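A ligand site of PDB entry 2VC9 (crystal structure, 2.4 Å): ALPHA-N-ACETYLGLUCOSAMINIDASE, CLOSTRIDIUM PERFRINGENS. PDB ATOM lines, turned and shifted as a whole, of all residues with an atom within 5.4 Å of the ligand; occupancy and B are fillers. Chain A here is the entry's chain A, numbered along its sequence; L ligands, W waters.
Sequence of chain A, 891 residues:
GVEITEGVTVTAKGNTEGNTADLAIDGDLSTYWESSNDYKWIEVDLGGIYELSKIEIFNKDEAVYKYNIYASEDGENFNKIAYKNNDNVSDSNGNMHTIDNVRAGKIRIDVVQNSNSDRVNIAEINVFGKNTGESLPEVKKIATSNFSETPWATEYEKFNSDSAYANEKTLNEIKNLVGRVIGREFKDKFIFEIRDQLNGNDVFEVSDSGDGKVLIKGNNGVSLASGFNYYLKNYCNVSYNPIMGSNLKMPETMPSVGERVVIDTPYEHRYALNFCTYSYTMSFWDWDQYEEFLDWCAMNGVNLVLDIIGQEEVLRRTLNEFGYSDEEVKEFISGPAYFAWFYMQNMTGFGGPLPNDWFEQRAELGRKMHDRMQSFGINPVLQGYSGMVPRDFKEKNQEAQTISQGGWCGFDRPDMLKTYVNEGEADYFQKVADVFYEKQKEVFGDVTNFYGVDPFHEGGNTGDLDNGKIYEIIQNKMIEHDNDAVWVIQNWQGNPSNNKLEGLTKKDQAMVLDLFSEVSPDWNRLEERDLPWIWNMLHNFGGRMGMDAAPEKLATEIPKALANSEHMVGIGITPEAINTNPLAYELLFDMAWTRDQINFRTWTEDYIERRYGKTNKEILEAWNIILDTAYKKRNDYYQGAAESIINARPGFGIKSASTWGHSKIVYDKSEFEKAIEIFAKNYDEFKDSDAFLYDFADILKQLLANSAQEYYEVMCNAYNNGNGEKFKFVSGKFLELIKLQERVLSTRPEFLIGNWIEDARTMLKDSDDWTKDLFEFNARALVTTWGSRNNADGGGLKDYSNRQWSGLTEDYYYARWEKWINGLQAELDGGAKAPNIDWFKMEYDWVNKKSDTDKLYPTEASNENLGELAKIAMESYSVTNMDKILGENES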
ATOM      1  N   ASN A 274      33.648 -30.833   1.420  1.00  0.00           N
ATOM      2  CA  ASN A 274      32.800 -31.111   0.267  1.00  0.00           C
ATOM      3  C   ASN A 274      33.753 -31.326  -0.906  1.00  0.00           C
ATOM      4  O   ASN A 274      34.918 -30.933  -0.828  1.00  0.00           O
ATOM      5  CB  ASN A 274      31.914 -29.888  -0.006  1.00  0.00           C
ATOM      6  CG  ASN A 274      30.696 -30.205  -0.870  1.00  0.00           C
ATOM      7  OD1 ASN A 274      30.819 -30.620  -2.027  1.00  0.00           O
ATOM      8  ND2 ASN A 274      29.506 -29.975  -0.308  1.00  0.00           N
ATOM      9  N   CYS A 276      33.180 -29.674  -3.527  1.00  0.00           N
ATOM     10  CA  CYS A 276      33.213 -28.263  -3.934  1.00  0.00           C
ATOM     11  C   CYS A 276      34.307 -27.438  -3.242  1.00  0.00           C
ATOM     12  O   CYS A 276      34.749 -26.418  -3.803  1.00  0.00           O
ATOM     13  CB  CYS A 276      31.846 -27.610  -3.750  1.00  0.00           C
ATOM     14  SG  CYS A 276      30.489 -28.401  -4.663  1.00  0.00           S
ATOM     15  N   TYR A 280      36.045 -24.050  -4.891  1.00  0.00           N
ATOM     16  CA  TYR A 280      35.784 -22.710  -4.362  1.00  0.00           C
ATOM     17  C   TYR A 280      36.863 -22.143  -3.417  1.00  0.00           C
ATOM     18  O   TYR A 280      37.055 -20.932  -3.380  1.00  0.00           O
ATOM     19  CB  TYR A 280      34.406 -22.635  -3.684  1.00  0.00           C
ATOM     20  CG  TYR A 280      33.250 -22.882  -4.636  1.00  0.00           C
ATOM     21  CD1 TYR A 280      33.166 -22.233  -5.866  1.00  0.00           C
ATOM     22  CD2 TYR A 280      32.230 -23.777  -4.296  1.00  0.00           C
ATOM     23  CE1 TYR A 280      32.113 -22.457  -6.738  1.00  0.00           C
ATOM     24  CE2 TYR A 280      31.171 -24.009  -5.158  1.00  0.00           C
ATOM     25  CZ  TYR A 280      31.117 -23.340  -6.366  1.00  0.00           C
ATOM     26  OH  TYR A 280      30.071 -23.567  -7.228  1.00  0.00           O
ATOM     27  N   TRP A 341      33.331 -30.708  -9.727  1.00  0.00           N
ATOM     28  CA  TRP A 341      32.269 -31.115 -10.646  1.00  0.00           C
ATOM     29  C   TRP A 341      32.714 -32.114 -11.681  1.00  0.00           C
ATOM     30  O   TRP A 341      31.902 -32.823 -12.268  1.00  0.00           O
ATOM     31  CB  TRP A 341      31.566 -29.865 -11.213  1.00  0.00           C
ATOM     32  CG  TRP A 341      31.222 -28.992 -10.071  1.00  0.00           C
ATOM     33  CD1 TRP A 341      30.188 -29.163  -9.206  1.00  0.00           C
ATOM     34  CD2 TRP A 341      31.968 -27.873  -9.583  1.00  0.00           C
ATOM     35  NE1 TRP A 341      30.218 -28.203  -8.230  1.00  0.00           N
ATOM     36  CE2 TRP A 341      31.311 -27.394  -8.443  1.00  0.00           C
ATOM     37  CE3 TRP A 341      33.134 -27.219 -10.015  1.00  0.00           C
ATOM     38  CZ2 TRP A 341      31.760 -26.294  -7.724  1.00  0.00           C
ATOM     39  CZ3 TRP A 341      33.573 -26.109  -9.295  1.00  0.00           C
ATOM     40  CH2 TRP A 341      32.888 -25.659  -8.171  1.00  0.00           C
ATOM     41  N   MET A 344      32.652 -35.341  -9.465  1.00  0.00           N
ATOM     42  CA  MET A 344      31.228 -35.639  -9.191  1.00  0.00           C
ATOM     43  C   MET A 344      30.426 -35.997 -10.439  1.00  0.00           C
ATOM     44  O   MET A 344      29.203 -36.110 -10.375  1.00  0.00           O
ATOM     45  CB  MET A 344      30.557 -34.524  -8.392  1.00  0.00           C
ATOM     46  CG  MET A 344      30.992 -34.528  -6.924  1.00  0.00           C
ATOM     47  SD  MET A 344      30.136 -33.412  -5.803  1.00  0.00           S
ATOM     48  CE  MET A 344      30.471 -31.797  -6.513  1.00  0.00           C
ATOM     49  N   ASN A 346      29.769 -34.431 -13.254  1.00  0.00           N
ATOM     50  CA  ASN A 346      28.860 -33.375 -13.706  1.00  0.00           C
ATOM     51  C   ASN A 346      29.305 -32.648 -14.978  1.00  0.00           C
ATOM     52  O   ASN A 346      28.463 -32.182 -15.743  1.00  0.00           O
ATOM     53  CB  ASN A 346      28.632 -32.358 -12.586  1.00  0.00           C
ATOM     54  CG  ASN A 346      27.895 -32.947 -11.383  1.00  0.00           C
ATOM     55  OD1 ASN A 346      26.935 -33.718 -11.525  1.00  0.00           O
ATOM     56  ND2 ASN A 346      28.308 -32.554 -10.199  1.00  0.00           N
ATOM     57  N   TRP A 408      24.313 -31.279 -17.204  1.00  0.00           N
ATOM     58  CA  TRP A 408      24.296 -30.668 -15.895  1.00  0.00           C
ATOM     59  C   TRP A 408      24.702 -29.225 -16.115  1.00  0.00           C
ATOM     60  O   TRP A 408      25.813 -28.937 -16.565  1.00  0.00           O
ATOM     61  CB  TRP A 408      25.275 -31.381 -14.961  1.00  0.00           C
ATOM     62  CG  TRP A 408      25.398 -30.781 -13.604  1.00  0.00           C
ATOM     63  CD1 TRP A 408      24.630 -31.056 -12.498  1.00  0.00           C
ATOM     64  CD2 TRP A 408      26.355 -29.804 -13.187  1.00  0.00           C
ATOM     65  NE1 TRP A 408      25.045 -30.303 -11.428  1.00  0.00           N
ATOM     66  CE2 TRP A 408      26.110 -29.521 -11.820  1.00  0.00           C
ATOM     67  CE3 TRP A 408      27.390 -29.120 -13.837  1.00  0.00           C
ATOM     68  CZ2 TRP A 408      26.867 -28.591 -11.093  1.00  0.00           C
ATOM     69  CZ3 TRP A 408      28.163 -28.194 -13.104  1.00  0.00           C
ATOM     70  CH2 TRP A 408      27.885 -27.946 -11.743  1.00  0.00           C
ATOM     71  N   HIS A 457      24.979 -37.985  -9.064  1.00  0.00           N
ATOM     72  CA  HIS A 457      24.983 -36.774  -8.275  1.00  0.00           C
ATOM     73  C   HIS A 457      24.353 -35.628  -9.072  1.00  0.00           C
ATOM     74  O   HIS A 457      24.866 -35.235 -10.114  1.00  0.00           O
ATOM     75  CB  HIS A 457      26.397 -36.419  -7.814  1.00  0.00           C
ATOM     76  CG  HIS A 457      26.463 -35.233  -6.890  1.00  0.00           C
ATOM     77  ND1 HIS A 457      26.312 -35.345  -5.532  1.00  0.00           N
ATOM     78  CD2 HIS A 457      26.645 -33.922  -7.145  1.00  0.00           C
ATOM     79  CE1 HIS A 457      26.402 -34.152  -4.973  1.00  0.00           C
ATOM     80  NE2 HIS A 457      26.603 -33.269  -5.937  1.00  0.00           N
ATOM     81  N   GLU A 458      23.229 -35.128  -8.561  1.00  0.00           N
ATOM     82  CA  GLU A 458      22.470 -34.027  -9.179  1.00  0.00           C
ATOM     83  C   GLU A 458      22.078 -34.278 -10.636  1.00  0.00           C
ATOM     84  O   GLU A 458      22.140 -33.366 -11.470  1.00  0.00           O
ATOM     85  CB  GLU A 458      23.171 -32.677  -9.010  1.00  0.00           C
ATOM     86  CG  GLU A 458      23.206 -32.153  -7.586  1.00  0.00           C
ATOM     87  CD  GLU A 458      23.668 -30.710  -7.523  1.00  0.00           C
ATOM     88  OE1 GLU A 458      24.320 -30.257  -8.497  1.00  0.00           O
ATOM     89  OE2 GLU A 458      23.379 -30.039  -6.507  1.00  0.00           O
ATOM     90  N   GLN A 490      27.766 -39.503  -0.368  1.00  0.00           N
ATOM     91  CA  GLN A 490      27.068 -38.254  -0.021  1.00  0.00           C
ATOM     92  C   GLN A 490      25.557 -38.473  -0.021  1.00  0.00           C
ATOM     93  O   GLN A 490      25.045 -39.187  -0.883  1.00  0.00           O
ATOM     94  CB  GLN A 490      27.383 -37.147  -1.009  1.00  0.00           C
ATOM     95  CG  GLN A 490      28.779 -36.606  -1.016  1.00  0.00           C
ATOM     96  CD  GLN A 490      28.911 -35.456  -1.998  1.00  0.00           C
ATOM     97  OE1 GLN A 490      28.441 -34.353  -1.732  1.00  0.00           O
ATOM     98  NE2 GLN A 490      29.523 -35.725  -3.144  1.00  0.00           N
ATOM     99  N   TRP A 492      22.594 -36.169  -0.650  1.00  0.00           N
ATOM    100  CA  TRP A 492      22.199 -34.848  -1.098  1.00  0.00           C
ATOM    101  C   TRP A 492      20.800 -34.878  -1.716  1.00  0.00           C
ATOM    102  O   TRP A 492      20.566 -35.569  -2.694  1.00  0.00           O
ATOM    103  CB  TRP A 492      23.259 -34.232  -2.041  1.00  0.00           C
ATOM    104  CG  TRP A 492      22.930 -32.856  -2.584  1.00  0.00           C
ATOM    105  CD1 TRP A 492      22.873 -32.503  -3.890  1.00  0.00           C
ATOM    106  CD2 TRP A 492      22.627 -31.668  -1.832  1.00  0.00           C
ATOM    107  NE1 TRP A 492      22.549 -31.169  -4.018  1.00  0.00           N
ATOM    108  CE2 TRP A 492      22.382 -30.631  -2.773  1.00  0.00           C
ATOM    109  CE3 TRP A 492      22.533 -31.370  -0.461  1.00  0.00           C
ATOM    110  CZ2 TRP A 492      22.052 -29.315  -2.380  1.00  0.00           C
ATOM    111  CZ3 TRP A 492      22.201 -30.046  -0.073  1.00  0.00           C
ATOM    112  CH2 TRP A 492      21.960 -29.043  -1.035  1.00  0.00           C
ATOM    113  N   LEU A 515      24.585 -34.567   4.406  1.00  0.00           N
ATOM    114  CA  LEU A 515      25.335 -33.375   3.976  1.00  0.00           C
ATOM    115  C   LEU A 515      24.925 -32.079   4.654  1.00  0.00           C
ATOM    116  O   LEU A 515      25.770 -31.221   4.894  1.00  0.00           O
ATOM    117  CB  LEU A 515      25.233 -33.212   2.464  1.00  0.00           C
ATOM    118  CG  LEU A 515      26.511 -32.861   1.687  1.00  0.00           C
ATOM    119  CD1 LEU A 515      27.491 -34.037   1.656  1.00  0.00           C
ATOM    120  CD2 LEU A 515      26.169 -32.412   0.279  1.00  0.00           C
ATOM    121  N   LEU A 538      26.885 -28.199   6.602  1.00  0.00           N
ATOM    122  CA  LEU A 538      27.278 -27.711   5.286  1.00  0.00           C
ATOM    123  C   LEU A 538      27.588 -26.212   5.365  1.00  0.00           C
ATOM    124  O   LEU A 538      28.691 -25.787   5.053  1.00  0.00           O
ATOM    125  CB  LEU A 538      26.154 -28.001   4.267  1.00  0.00           C
ATOM    126  CG  LEU A 538      26.437 -28.142   2.763  1.00  0.00           C
ATOM    127  CD1 LEU A 538      25.191 -28.662   2.029  1.00  0.00           C
ATOM    128  CD2 LEU A 538      26.937 -26.822   2.149  1.00  0.00           C
ATOM    129  N   PHE A 541      27.575 -22.079   0.931  1.00  0.00           N
ATOM    130  CA  PHE A 541      27.348 -22.438  -0.454  1.00  0.00           C
ATOM    131  C   PHE A 541      28.126 -21.514  -1.381  1.00  0.00           C
ATOM    132  O   PHE A 541      28.015 -20.278  -1.277  1.00  0.00           O
ATOM    133  CB  PHE A 541      25.854 -22.412  -0.773  1.00  0.00           C
ATOM    134  CG  PHE A 541      25.083 -23.554  -0.187  1.00  0.00           C
ATOM    135  CD1 PHE A 541      24.638 -24.593  -0.986  1.00  0.00           C
ATOM    136  CD2 PHE A 541      24.786 -23.594   1.172  1.00  0.00           C
ATOM    137  CE1 PHE A 541      23.897 -25.670  -0.443  1.00  0.00           C
ATOM    138  CE2 PHE A 541      24.063 -24.662   1.723  1.00  0.00           C
ATOM    139  CZ  PHE A 541      23.617 -25.691   0.902  1.00  0.00           C
ATOM    140  N   THR A 574      30.750 -30.071   5.709  1.00  0.00           N
ATOM    141  CA  THR A 574      30.677 -30.283   4.269  1.00  0.00           C
ATOM    142  C   THR A 574      30.531 -28.956   3.503  1.00  0.00           C
ATOM    143  O   THR A 574      29.713 -28.859   2.602  1.00  0.00           O
ATOM    144  CB  THR A 574      29.531 -31.257   3.894  1.00  0.00           C
ATOM    145  OG1 THR A 574      28.305 -30.809   4.480  1.00  0.00           O
ATOM    146  CG2 THR A 574      29.812 -32.680   4.376  1.00  0.00           C
ATOM    147  N   GLU A 576      31.048 -25.815   0.952  1.00  0.00           N
ATOM    148  CA  GLU A 576      31.460 -25.703  -0.433  1.00  0.00           C
ATOM    149  C   GLU A 576      32.686 -24.800  -0.539  1.00  0.00           C
ATOM    150  O   GLU A 576      33.429 -24.859  -1.518  1.00  0.00           O
ATOM    151  CB  GLU A 576      30.295 -25.213  -1.288  1.00  0.00           C
ATOM    152  CG  GLU A 576      29.122 -26.187  -1.287  1.00  0.00           C
ATOM    153  CD  GLU A 576      27.993 -25.815  -2.260  1.00  0.00           C
ATOM    154  OE1 GLU A 576      27.995 -24.731  -2.896  1.00  0.00           O
ATOM    155  OE2 GLU A 576      27.061 -26.641  -2.366  1.00  0.00           O
ATOM    156  N   GLN A 639      19.847 -21.826   1.369  1.00  0.00           N
ATOM    157  CA  GLN A 639      21.182 -22.275   0.981  1.00  0.00           C
ATOM    158  C   GLN A 639      22.229 -21.176   1.145  1.00  0.00           C
ATOM    159  O   GLN A 639      22.443 -20.357   0.249  1.00  0.00           O
ATOM    160  CB  GLN A 639      21.174 -22.842  -0.447  1.00  0.00           C
ATOM    161  CG  GLN A 639      20.368 -24.139  -0.604  1.00  0.00           C
ATOM    162  CD  GLN A 639      20.636 -24.843  -1.934  1.00  0.00           C
ATOM    163  OE1 GLN A 639      21.445 -24.398  -2.743  1.00  0.00           O
ATOM    164  NE2 GLN A 639      19.959 -25.959  -2.138  1.00  0.00           N
ATOM    165  N   TRP A 786      30.849 -18.463 -13.939  1.00  0.00           N
ATOM    166  CA  TRP A 786      31.000 -19.908 -13.665  1.00  0.00           C
ATOM    167  C   TRP A 786      31.470 -20.704 -14.890  1.00  0.00           C
ATOM    168  O   TRP A 786      32.590 -21.217 -14.914  1.00  0.00           O
ATOM    169  CB  TRP A 786      29.730 -20.488 -13.044  1.00  0.00           C
ATOM    170  CG  TRP A 786      29.977 -21.599 -12.048  1.00  0.00           C
ATOM    171  CD1 TRP A 786      29.886 -21.514 -10.680  1.00  0.00           C
ATOM    172  CD2 TRP A 786      30.337 -22.951 -12.334  1.00  0.00           C
ATOM    173  NE1 TRP A 786      30.173 -22.731 -10.108  1.00  0.00           N
ATOM    174  CE2 TRP A 786      30.452 -23.630 -11.105  1.00  0.00           C
ATOM    175  CE3 TRP A 786      30.579 -23.662 -13.520  1.00  0.00           C
ATOM    176  CZ2 TRP A 786      30.792 -24.976 -11.024  1.00  0.00           C
ATOM    177  CZ3 TRP A 786      30.932 -25.004 -13.438  1.00  0.00           C
ATOM    178  CH2 TRP A 786      31.034 -25.644 -12.200  1.00  0.00           C
ATOM    179  N   LEU A 797      23.926 -21.007 -13.490  1.00  0.00           N
ATOM    180  CA  LEU A 797      25.128 -20.881 -12.645  1.00  0.00           C
ATOM    181  C   LEU A 797      25.743 -19.475 -12.525  1.00  0.00           C
ATOM    182  O   LEU A 797      26.737 -19.302 -11.819  1.00  0.00           O
ATOM    183  CB  LEU A 797      26.214 -21.857 -13.088  1.00  0.00           C
ATOM    184  CG  LEU A 797      25.990 -23.366 -12.872  1.00  0.00           C
ATOM    185  CD1 LEU A 797      27.055 -24.118 -13.633  1.00  0.00           C
ATOM    186  CD2 LEU A 797      26.022 -23.735 -11.401  1.00  0.00           C
ATOM    187  N   TYR A 800      26.988 -17.862  -9.042  1.00  0.00           N
ATOM    188  CA  TYR A 800      26.732 -18.858  -8.008  1.00  0.00           C
ATOM    189  C   TYR A 800      27.755 -18.681  -6.898  1.00  0.00           C
ATOM    190  O   TYR A 800      27.445 -18.827  -5.715  1.00  0.00           O
ATOM    191  CB  TYR A 800      26.746 -20.303  -8.574  1.00  0.00           C
ATOM    192  CG  TYR A 800      26.467 -21.336  -7.493  1.00  0.00           C
ATOM    193  CD1 TYR A 800      25.181 -21.796  -7.249  1.00  0.00           C
ATOM    194  CD2 TYR A 800      27.494 -21.816  -6.685  1.00  0.00           C
ATOM    195  CE1 TYR A 800      24.922 -22.722  -6.235  1.00  0.00           C
ATOM    196  CE2 TYR A 800      27.256 -22.740  -5.675  1.00  0.00           C
ATOM    197  CZ  TYR A 800      25.969 -23.189  -5.453  1.00  0.00           C
ATOM    198  OH  TYR A 800      25.743 -24.100  -4.447  1.00  0.00           O
HETATM  199  C1  LIG L   1      27.496 -25.296  -8.813  1.00  0.00           C
HETATM  200  C2  LIG L   1      27.643 -25.909  -7.423  1.00  0.00           C
HETATM  201  O1  LIG L   1      28.598 -25.572  -6.723  1.00  0.00           O
HETATM  202  N1  LIG L   1      26.705 -26.781  -7.076  1.00  0.00           N
HETATM  203  C3  LIG L   1      26.676 -27.450  -5.773  1.00  0.00           C
HETATM  204  C4  LIG L   1      25.320 -27.165  -5.109  1.00  0.00           C
HETATM  205  N2  LIG L   1      25.302 -27.755  -3.755  1.00  0.00           N
HETATM  206  C5  LIG L   1      25.567 -29.221  -3.687  1.00  0.00           C
HETATM  207  C6  LIG L   1      25.714 -29.653  -2.228  1.00  0.00           C
HETATM  208  O2  LIG L   1      26.876 -29.077  -1.650  1.00  0.00           O
HETATM  209  C7  LIG L   1      26.824 -29.632  -4.488  1.00  0.00           C
HETATM  210  O3  LIG L   1      26.849 -31.065  -4.569  1.00  0.00           O
HETATM  211  C8  LIG L   1      26.876 -28.964  -5.883  1.00  0.00           C
HETATM  212  O4  LIG L   1      28.103 -29.261  -6.556  1.00  0.00           O
HETATM  213  O   HOH W   1      27.240 -31.104  -8.310  1.00  0.00           O
HETATM  214  O   HOH W   2      22.803 -26.341  -3.890  1.00  0.00           O
HETATM  215  O   HOH W   3      28.910 -32.098  -3.124  1.00  0.00           O
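A nitrogen (N2) of the ligand is in salt-bridge range of the side-chain carboxylate of Glu 576 (2.5 Å).
The side-chain hydroxyl (OH) of Tyr 280 sits at hydrogen-bond distance from an oxygen (O1) of the ligand, at 2.5 Å.
NE2 of His 457 is in hydrogen-bond range of O3 of the ligand (2.6 Å).
NE1 of Trp 341 is in hydrogen-bond range of O4 of the ligand (2.9 Å).
O2 of the ligand is in hydrogen-bond range of ND2 of Asn 274.
An oxygen (O4) of the ligand is in hydrogen-bond range of the side-chain sulfur (SG) of Cys 276 (3.2 Å).
NE1 of Trp 786 sits at hydrogen-bond distance from OH of Tyr 280 (3.0 Å).
A ring nitrogen (NE2) of His 457 is in hydrogen-bond range of the side-chain sulfur (SD) of Met 344, at 3.5 Å.
The backbone carbonyl oxygen (O) of His 457 lies close to the side-chain amide oxygen (OD1) of Asn 346 (2.9 Å).
N of Asn 346 is in hydrogen-bond range of O of Trp 341, 2.8 Å away.
SD of Met 344 sits at hydrogen-bond distance from NE2 of Gln 490 (3.6 Å).
O of Met 344 sits close to OD1 of Asn 346, at 3.5 Å.
The indole nitrogen of Trp 408 lies within hydrogen-bond range of the side-chain carboxylate of Glu 458 (3.0 Å).
The backbone carbonyl oxygen (O) of Leu 515 is in hydrogen-bond range of the side-chain hydroxyl (OG1) of Thr 574 (2.6 Å).
Residues that only touch the ligand: Met 344, Trp 408, Glu 458, Trp 492, Leu 515, Trp 786, Leu 797 and Tyr 800.
Hydrophobic or aromatic side chains that line the ligand: Tyr 280, Trp 341, Met 344, Trp 408, His 457, Trp 492, Leu 515, Trp 786, Leu 797 and Tyr 800.
Water W1 lies within hydrogen-bond range of the side-chain amide nitrogen (ND2) of Asn 346 (2.6 Å), an oxygen (O4) of the ligand (2.7 Å), the side-chain carboxylate (OE1) of Glu 458 (3.0 Å) and a ring nitrogen (NE2) of His 457 (3.3 Å).
Water W2 lies within hydrogen-bond range of the side-chain amide oxygen of Gln 639 (2.6 Å) and a nitrogen (N2) of the ligand (2.9 Å).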
